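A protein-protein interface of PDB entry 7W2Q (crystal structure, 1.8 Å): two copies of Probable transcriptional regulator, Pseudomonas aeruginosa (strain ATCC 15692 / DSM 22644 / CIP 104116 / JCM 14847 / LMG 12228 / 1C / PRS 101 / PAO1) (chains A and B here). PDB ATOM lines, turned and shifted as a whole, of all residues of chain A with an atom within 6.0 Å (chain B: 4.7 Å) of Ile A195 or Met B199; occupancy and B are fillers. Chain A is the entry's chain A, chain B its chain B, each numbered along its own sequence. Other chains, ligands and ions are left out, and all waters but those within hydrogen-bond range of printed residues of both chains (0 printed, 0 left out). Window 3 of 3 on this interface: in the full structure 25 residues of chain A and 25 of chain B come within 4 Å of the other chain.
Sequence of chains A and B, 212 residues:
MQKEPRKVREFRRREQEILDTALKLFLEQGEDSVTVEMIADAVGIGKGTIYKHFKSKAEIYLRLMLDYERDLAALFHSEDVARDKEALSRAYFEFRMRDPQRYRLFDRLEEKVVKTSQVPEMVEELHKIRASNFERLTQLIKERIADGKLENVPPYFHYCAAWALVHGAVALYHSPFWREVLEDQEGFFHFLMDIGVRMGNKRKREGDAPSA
Of the 12 printed residues of chain A, 3 touch a printed residue of chain B. Hydrophobic or aromatic side chains of chain A that line the printed part of chain B: Phe A191, Ile A195 and Met A199. Among the printed residues, no Asp or Glu carboxylate lies within 4 Å of a Lys or Arg side-chain nitrogen of the other chain.
Of the printed residues of chain B, Phe A191 touches His B158. Ile A195 touches just these residues of chain B: Ala B161 (3.6 Å) and Met B199 (3.5 Å). Of the printed residues of chain B, Met A199 touches Ile B195 (3.6 Å). Of the printed residues of chain A, His B158 touches Phe A191. Of the printed residues of chain A, Ala B161 touches Ile A195. Of the printed residues of chain A, Ile B195 touches Met A199 (3.6 Å). Met B199 touches one residue of chain A. The nearest printed residue of chain A that does not touch His B158 is Ile A195 (6.1 Å).
Ile A195 touches Met B199, and with the chains exchanged Met A199 touches Ile B195. Positions printed for both chains: 165, 195, 196, 197, 198 and 199.
Among the printed residues, merely in contact across the chains: Ile A195 with Met B199 (3.5 Å), Met A199 with Ile B195 (3.6 Å), Ile A195 with Ala B161 (3.6 Å) and Phe A191 with His B158 (3.7 Å).
The side-chain amide oxygen (OD1) of Asn B201 sits close to the backbone carbonyl oxygen (O) of Met B199.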
ATOM      1  N   ARG A  90     -34.540 -15.125  16.486  1.00  0.00           N
ATOM      2  CA  ARG A  90     -33.420 -15.351  15.576  1.00  0.00           C
ATOM      3  C   ARG A  90     -33.567 -14.531  14.304  1.00  0.00           C
ATOM      4  O   ARG A  90     -32.595 -13.925  13.827  1.00  0.00           O
ATOM      5  CB  ARG A  90     -33.307 -16.837  15.248  1.00  0.00           C
ATOM      6  CG  ARG A  90     -32.053 -17.166  14.473  1.00  0.00           C
ATOM      7  CD  ARG A  90     -31.844 -18.670  14.319  1.00  0.00           C
ATOM      8  NE  ARG A  90     -30.536 -18.929  13.730  1.00  0.00           N
ATOM      9  CZ  ARG A  90     -29.416 -19.036  14.429  1.00  0.00           C
ATOM     10  NH1 ARG A  90     -29.411 -18.926  15.748  1.00  0.00           N
ATOM     11  NH2 ARG A  90     -28.269 -19.251  13.791  1.00  0.00           N
ATOM     12  N   LEU A 165     -25.465  -5.754  21.339  1.00  0.00           N
ATOM     13  CA  LEU A 165     -24.878  -6.801  20.505  1.00  0.00           C
ATOM     14  C   LEU A 165     -24.933  -6.428  19.030  1.00  0.00           C
ATOM     15  O   LEU A 165     -23.937  -6.558  18.305  1.00  0.00           O
ATOM     16  CB  LEU A 165     -25.607  -8.122  20.759  1.00  0.00           C
ATOM     17  CG  LEU A 165     -25.042  -9.289  19.949  1.00  0.00           C
ATOM     18  CD1 LEU A 165     -23.645  -9.638  20.435  1.00  0.00           C
ATOM     19  CD2 LEU A 165     -25.983 -10.473  20.063  1.00  0.00           C
ATOM     20  N   HIS A 190     -23.755 -16.970  11.877  1.00  0.00           N
ATOM     21  CA  HIS A 190     -24.764 -17.742  12.590  1.00  0.00           C
ATOM     22  C   HIS A 190     -24.397 -17.914  14.057  1.00  0.00           C
ATOM     23  O   HIS A 190     -25.289 -18.021  14.909  1.00  0.00           O
ATOM     24  CB  HIS A 190     -24.968 -19.084  11.891  1.00  0.00           C
ATOM     25  CG  HIS A 190     -25.896 -18.993  10.720  1.00  0.00           C
ATOM     26  ND1 HIS A 190     -25.618 -18.218   9.613  1.00  0.00           N
ATOM     27  CD2 HIS A 190     -27.108 -19.550  10.495  1.00  0.00           C
ATOM     28  CE1 HIS A 190     -26.615 -18.313   8.750  1.00  0.00           C
ATOM     29  NE2 HIS A 190     -27.531 -19.117   9.260  1.00  0.00           N
ATOM     30  N   PHE A 191     -23.098 -17.926  14.361  1.00  0.00           N
ATOM     31  CA  PHE A 191     -22.636 -17.922  15.744  1.00  0.00           C
ATOM     32  C   PHE A 191     -23.124 -16.680  16.481  1.00  0.00           C
ATOM     33  O   PHE A 191     -23.605 -16.776  17.619  1.00  0.00           O
ATOM     34  CB  PHE A 191     -21.107 -18.010  15.753  1.00  0.00           C
ATOM     35  CG  PHE A 191     -20.481 -17.968  17.121  1.00  0.00           C
ATOM     36  CD1 PHE A 191     -20.498 -19.083  17.946  1.00  0.00           C
ATOM     37  CD2 PHE A 191     -19.814 -16.828  17.543  1.00  0.00           C
ATOM     38  CE1 PHE A 191     -19.902 -19.049  19.199  1.00  0.00           C
ATOM     39  CE2 PHE A 191     -19.199 -16.796  18.790  1.00  0.00           C
ATOM     40  CZ  PHE A 191     -19.247 -17.892  19.609  1.00  0.00           C
ATOM     41  N   LEU A 192     -23.023 -15.509  15.846  1.00  0.00           N
ATOM     42  CA  LEU A 192     -23.539 -14.287  16.465  1.00  0.00           C
ATOM     43  C   LEU A 192     -25.049 -14.364  16.658  1.00  0.00           C
ATOM     44  O   LEU A 192     -25.575 -13.910  17.687  1.00  0.00           O
ATOM     45  CB  LEU A 192     -23.169 -13.065  15.618  1.00  0.00           C
ATOM     46  CG  LEU A 192     -21.770 -12.480  15.817  1.00  0.00           C
ATOM     47  CD1 LEU A 192     -21.618 -11.220  14.981  1.00  0.00           C
ATOM     48  CD2 LEU A 192     -21.477 -12.190  17.288  1.00  0.00           C
ATOM     49  N   MET A 193     -25.772 -14.911  15.671  1.00  0.00           N
ATOM     50  CA  MET A 193     -27.222 -15.051  15.803  1.00  0.00           C
ATOM     51  C   MET A 193     -27.574 -15.965  16.967  1.00  0.00           C
ATOM     52  O   MET A 193     -28.507 -15.685  17.730  1.00  0.00           O
ATOM     53  CB  MET A 193     -27.824 -15.600  14.511  1.00  0.00           C
ATOM     54  CG  MET A 193     -28.123 -14.562  13.448  1.00  0.00           C
ATOM     55  SD  MET A 193     -28.335 -15.317  11.827  1.00  0.00           S
ATOM     56  CE  MET A 193     -29.761 -16.342  12.093  1.00  0.00           C
ATOM     57  N   ASP A 194     -26.846 -17.075  17.107  1.00  0.00           N
ATOM     58  CA  ASP A 194     -27.059 -17.976  18.237  1.00  0.00           C
ATOM     59  C   ASP A 194     -26.843 -17.247  19.551  1.00  0.00           C
ATOM     60  O   ASP A 194     -27.600 -17.439  20.515  1.00  0.00           O
ATOM     61  CB  ASP A 194     -26.102 -19.169  18.145  1.00  0.00           C
ATOM     62  CG  ASP A 194     -26.517 -20.187  17.103  1.00  0.00           C
ATOM     63  OD1 ASP A 194     -27.655 -20.115  16.601  1.00  0.00           O
ATOM     64  OD2 ASP A 194     -25.691 -21.072  16.787  1.00  0.00           O
ATOM     65  N   ILE A 195     -25.806 -16.413  19.610  1.00  0.00           N
ATOM     66  CA  ILE A 195     -25.511 -15.669  20.826  1.00  0.00           C
ATOM     67  C   ILE A 195     -26.655 -14.721  21.146  1.00  0.00           C
ATOM     68  O   ILE A 195     -27.073 -14.609  22.302  1.00  0.00           O
ATOM     69  CB  ILE A 195     -24.177 -14.918  20.682  1.00  0.00           C
ATOM     70  CG1 ILE A 195     -22.999 -15.862  20.922  1.00  0.00           C
ATOM     71  CG2 ILE A 195     -24.140 -13.708  21.620  1.00  0.00           C
ATOM     72  CD1 ILE A 195     -21.675 -15.245  20.576  1.00  0.00           C
ATOM     73  N   GLY A 196     -27.200 -14.061  20.120  1.00  0.00           N
ATOM     74  CA  GLY A 196     -28.298 -13.124  20.340  1.00  0.00           C
ATOM     75  C   GLY A 196     -29.528 -13.812  20.900  1.00  0.00           C
ATOM     76  O   GLY A 196     -30.172 -13.299  21.820  1.00  0.00           O
ATOM     77  N   VAL A 197     -29.872 -14.979  20.351  1.00  0.00           N
ATOM     78  CA  VAL A 197     -31.061 -15.699  20.814  1.00  0.00           C
ATOM     79  C   VAL A 197     -30.864 -16.222  22.231  1.00  0.00           C
ATOM     80  O   VAL A 197     -31.816 -16.292  23.024  1.00  0.00           O
ATOM     81  CB  VAL A 197     -31.414 -16.831  19.835  1.00  0.00           C
ATOM     82  CG1 VAL A 197     -32.608 -17.644  20.346  1.00  0.00           C
ATOM     83  CG2 VAL A 197     -31.703 -16.253  18.464  1.00  0.00           C
ATOM     84  N   ARG A 198     -29.642 -16.629  22.568  1.00  0.00           N
ATOM     85  CA  ARG A 198     -29.374 -17.185  23.889  1.00  0.00           C
ATOM     86  C   ARG A 198     -29.119 -16.115  24.949  1.00  0.00           C
ATOM     87  O   ARG A 198     -29.099 -16.440  26.138  1.00  0.00           O
ATOM     88  CB  ARG A 198     -28.190 -18.156  23.797  1.00  0.00           C
ATOM     89  CG  ARG A 198     -28.527 -19.403  22.997  1.00  0.00           C
ATOM     90  CD  ARG A 198     -27.342 -20.345  22.855  1.00  0.00           C
ATOM     91  NE  ARG A 198     -27.541 -21.286  21.758  1.00  0.00           N
ATOM     92  CZ  ARG A 198     -26.568 -21.959  21.158  1.00  0.00           C
ATOM     93  NH1 ARG A 198     -25.309 -21.846  21.546  1.00  0.00           N
ATOM     94  NH2 ARG A 198     -26.871 -22.790  20.164  1.00  0.00           N
ATOM     95  N   MET A 199     -28.946 -14.852  24.552  1.00  0.00           N
ATOM     96  CA  MET A 199     -28.662 -13.794  25.509  1.00  0.00           C
ATOM     97  C   MET A 199     -29.785 -13.666  26.533  1.00  0.00           C
ATOM     98  O   MET A 199     -30.961 -13.628  26.173  1.00  0.00           O
ATOM     99  CB  MET A 199     -28.473 -12.462  24.764  1.00  0.00           C
ATOM    100  CG  MET A 199     -27.610 -11.484  25.477  1.00  0.00           C
ATOM    101  SD  MET A 199     -26.931 -10.258  24.325  1.00  0.00           S
ATOM    102  CE  MET A 199     -28.302 -10.001  23.241  1.00  0.00           C
ATOM    103  N   PHE B  93     -14.668  -8.514  31.455  1.00  0.00           N
ATOM    104  CA  PHE B  93     -15.806  -7.736  30.969  1.00  0.00           C
ATOM    105  C   PHE B  93     -16.071  -6.524  31.856  1.00  0.00           C
ATOM    106  O   PHE B  93     -16.426  -5.451  31.356  1.00  0.00           O
ATOM    107  CB  PHE B  93     -17.049  -8.623  30.858  1.00  0.00           C
ATOM    108  CG  PHE B  93     -17.057  -9.478  29.629  1.00  0.00           C
ATOM    109  CD1 PHE B  93     -17.220  -8.902  28.374  1.00  0.00           C
ATOM    110  CD2 PHE B  93     -16.867 -10.847  29.714  1.00  0.00           C
ATOM    111  CE1 PHE B  93     -17.213  -9.678  27.228  1.00  0.00           C
ATOM    112  CE2 PHE B  93     -16.866 -11.627  28.573  1.00  0.00           C
ATOM    113  CZ  PHE B  93     -17.022 -11.044  27.325  1.00  0.00           C
ATOM    114  N   LEU B 150     -16.632 -23.328  26.819  1.00  0.00           N
ATOM    115  CA  LEU B 150     -16.998 -22.594  25.619  1.00  0.00           C
ATOM    116  C   LEU B 150     -17.164 -23.551  24.446  1.00  0.00           C
ATOM    117  O   LEU B 150     -16.507 -24.596  24.373  1.00  0.00           O
ATOM    118  CB  LEU B 150     -15.936 -21.535  25.273  1.00  0.00           C
ATOM    119  CG  LEU B 150     -15.870 -20.298  26.170  1.00  0.00           C
ATOM    120  CD1 LEU B 150     -14.707 -19.400  25.716  1.00  0.00           C
ATOM    121  CD2 LEU B 150     -17.179 -19.514  26.149  1.00  0.00           C
ATOM    122  N   HIS B 158     -15.143 -16.353  19.513  1.00  0.00           N
ATOM    123  CA  HIS B 158     -15.367 -15.839  20.855  1.00  0.00           C
ATOM    124  C   HIS B 158     -14.745 -14.462  21.036  1.00  0.00           C
ATOM    125  O   HIS B 158     -15.341 -13.593  21.675  1.00  0.00           O
ATOM    126  CB  HIS B 158     -14.797 -16.812  21.885  1.00  0.00           C
ATOM    127  CG  HIS B 158     -15.464 -18.147  21.878  1.00  0.00           C
ATOM    128  ND1 HIS B 158     -16.750 -18.338  22.337  1.00  0.00           N
ATOM    129  CD2 HIS B 158     -15.019 -19.367  21.476  1.00  0.00           C
ATOM    130  CE1 HIS B 158     -17.070 -19.616  22.223  1.00  0.00           C
ATOM    131  NE2 HIS B 158     -16.039 -20.260  21.703  1.00  0.00           N
ATOM    132  N   ALA B 161     -17.002 -11.899  19.329  1.00  0.00           N
ATOM    133  CA  ALA B 161     -18.245 -11.695  20.073  1.00  0.00           C
ATOM    134  C   ALA B 161     -18.011 -10.808  21.290  1.00  0.00           C
ATOM    135  O   ALA B 161     -18.812  -9.908  21.578  1.00  0.00           O
ATOM    136  CB  ALA B 161     -18.836 -13.039  20.485  1.00  0.00           C
ATOM    137  N   ALA B 162     -16.919 -11.050  22.018  1.00  0.00           N
ATOM    138  CA  ALA B 162     -16.603 -10.234  23.185  1.00  0.00           C
ATOM    139  C   ALA B 162     -16.337  -8.794  22.776  1.00  0.00           C
ATOM    140  O   ALA B 162     -16.791  -7.858  23.441  1.00  0.00           O
ATOM    141  CB  ALA B 162     -15.393 -10.802  23.924  1.00  0.00           C
ATOM    142  N   LEU B 165     -19.776  -7.153  21.986  1.00  0.00           N
ATOM    143  CA  LEU B 165     -20.590  -6.839  23.162  1.00  0.00           C
ATOM    144  C   LEU B 165     -20.045  -5.617  23.901  1.00  0.00           C
ATOM    145  O   LEU B 165     -20.808  -4.697  24.263  1.00  0.00           O
ATOM    146  CB  LEU B 165     -20.668  -8.069  24.086  1.00  0.00           C
ATOM    147  CG  LEU B 165     -21.486  -7.841  25.360  1.00  0.00           C
ATOM    148  CD1 LEU B 165     -22.953  -7.645  25.015  1.00  0.00           C
ATOM    149  CD2 LEU B 165     -21.298  -9.040  26.314  1.00  0.00           C
ATOM    150  N   ILE B 195     -23.966 -11.666  30.851  1.00  0.00           N
ATOM    151  CA  ILE B 195     -24.158 -11.998  29.442  1.00  0.00           C
ATOM    152  C   ILE B 195     -22.811 -12.264  28.783  1.00  0.00           C
ATOM    153  O   ILE B 195     -22.647 -13.238  28.040  1.00  0.00           O
ATOM    154  CB  ILE B 195     -24.927 -10.873  28.731  1.00  0.00           C
ATOM    155  CG1 ILE B 195     -26.436 -11.020  28.963  1.00  0.00           C
ATOM    156  CG2 ILE B 195     -24.586 -10.837  27.241  1.00  0.00           C
ATOM    157  CD1 ILE B 195     -27.189  -9.745  28.646  1.00  0.00           C
ATOM    158  N   GLY B 196     -21.816 -11.427  29.087  1.00  0.00           N
ATOM    159  CA  GLY B 196     -20.497 -11.612  28.498  1.00  0.00           C
ATOM    160  C   GLY B 196     -19.872 -12.929  28.912  1.00  0.00           C
ATOM    161  O   GLY B 196     -19.306 -13.644  28.084  1.00  0.00           O
ATOM    162  N   VAL B 197     -19.989 -13.281  30.198  1.00  0.00           N
ATOM    163  CA  VAL B 197     -19.402 -14.531  30.677  1.00  0.00           C
ATOM    164  C   VAL B 197     -20.122 -15.727  30.065  1.00  0.00           C
ATOM    165  O   VAL B 197     -19.503 -16.767  29.767  1.00  0.00           O
ATOM    166  CB  VAL B 197     -19.444 -14.565  32.217  1.00  0.00           C
ATOM    167  CG1 VAL B 197     -18.983 -15.922  32.750  1.00  0.00           C
ATOM    168  CG2 VAL B 197     -18.618 -13.420  32.799  1.00  0.00           C
ATOM    169  N   ARG B 198     -21.441 -15.613  29.877  1.00  0.00           N
ATOM    170  CA  ARG B 198     -22.224 -16.733  29.365  1.00  0.00           C
ATOM    171  C   ARG B 198     -22.180 -16.832  27.853  1.00  0.00           C
ATOM    172  O   ARG B 198     -22.646 -17.830  27.303  1.00  0.00           O
ATOM    173  CB  ARG B 198     -23.700 -16.621  29.771  1.00  0.00           C
ATOM    174  CG  ARG B 198     -23.961 -16.641  31.251  1.00  0.00           C
ATOM    175  CD  ARG B 198     -25.442 -16.850  31.539  1.00  0.00           C
ATOM    176  NE  ARG B 198     -25.919 -16.262  32.788  1.00  0.00           N
ATOM    177  CZ  ARG B 198     -25.453 -16.554  33.996  1.00  0.00           C
ATOM    178  NH1 ARG B 198     -24.395 -17.332  34.163  1.00  0.00           N
ATOM    179  NH2 ARG B 198     -26.095 -16.096  35.068  1.00  0.00           N
ATOM    180  N   MET B 199     -21.660 -15.809  27.175  1.00  0.00           N
ATOM    181  CA  MET B 199     -21.647 -15.800  25.723  1.00  0.00           C
ATOM    182  C   MET B 199     -20.856 -16.980  25.172  1.00  0.00           C
ATOM    183  O   MET B 199     -19.712 -17.214  25.569  1.00  0.00           O
ATOM    184  CB  MET B 199     -21.029 -14.491  25.236  1.00  0.00           C
ATOM    185  CG  MET B 199     -21.467 -14.056  23.884  1.00  0.00           C
ATOM    186  SD  MET B 199     -21.261 -12.275  23.688  1.00  0.00           S
ATOM    187  CE  MET B 199     -19.638 -12.016  24.294  1.00  0.00           C
ATOM    188  N   GLY B 200     -21.459 -17.705  24.237  1.00  0.00           N
ATOM    189  CA  GLY B 200     -20.759 -18.821  23.621  1.00  0.00           C
ATOM    190  C   GLY B 200     -20.549 -20.023  24.513  1.00  0.00           C
ATOM    191  O   GLY B 200     -19.756 -20.909  24.159  1.00  0.00           O
ATOM    192  N   ASN B 201     -21.212 -20.076  25.668  1.00  0.00           N
ATOM    193  CA  ASN B 201     -21.090 -21.236  26.548  1.00  0.00           C
ATOM    194  C   ASN B 201     -21.673 -22.472  25.882  1.00  0.00           C
ATOM    195  O   ASN B 201     -22.684 -22.406  25.173  1.00  0.00           O
ATOM    196  CB  ASN B 201     -21.795 -20.984  27.880  1.00  0.00           C
ATOM    197  CG  ASN B 201     -21.059 -19.990  28.754  1.00  0.00           C
ATOM    198  OD1 ASN B 201     -20.163 -19.276  28.296  1.00  0.00           O
ATOM    199  ND2 ASN B 201     -21.441 -19.927  30.019  1.00  0.00           N
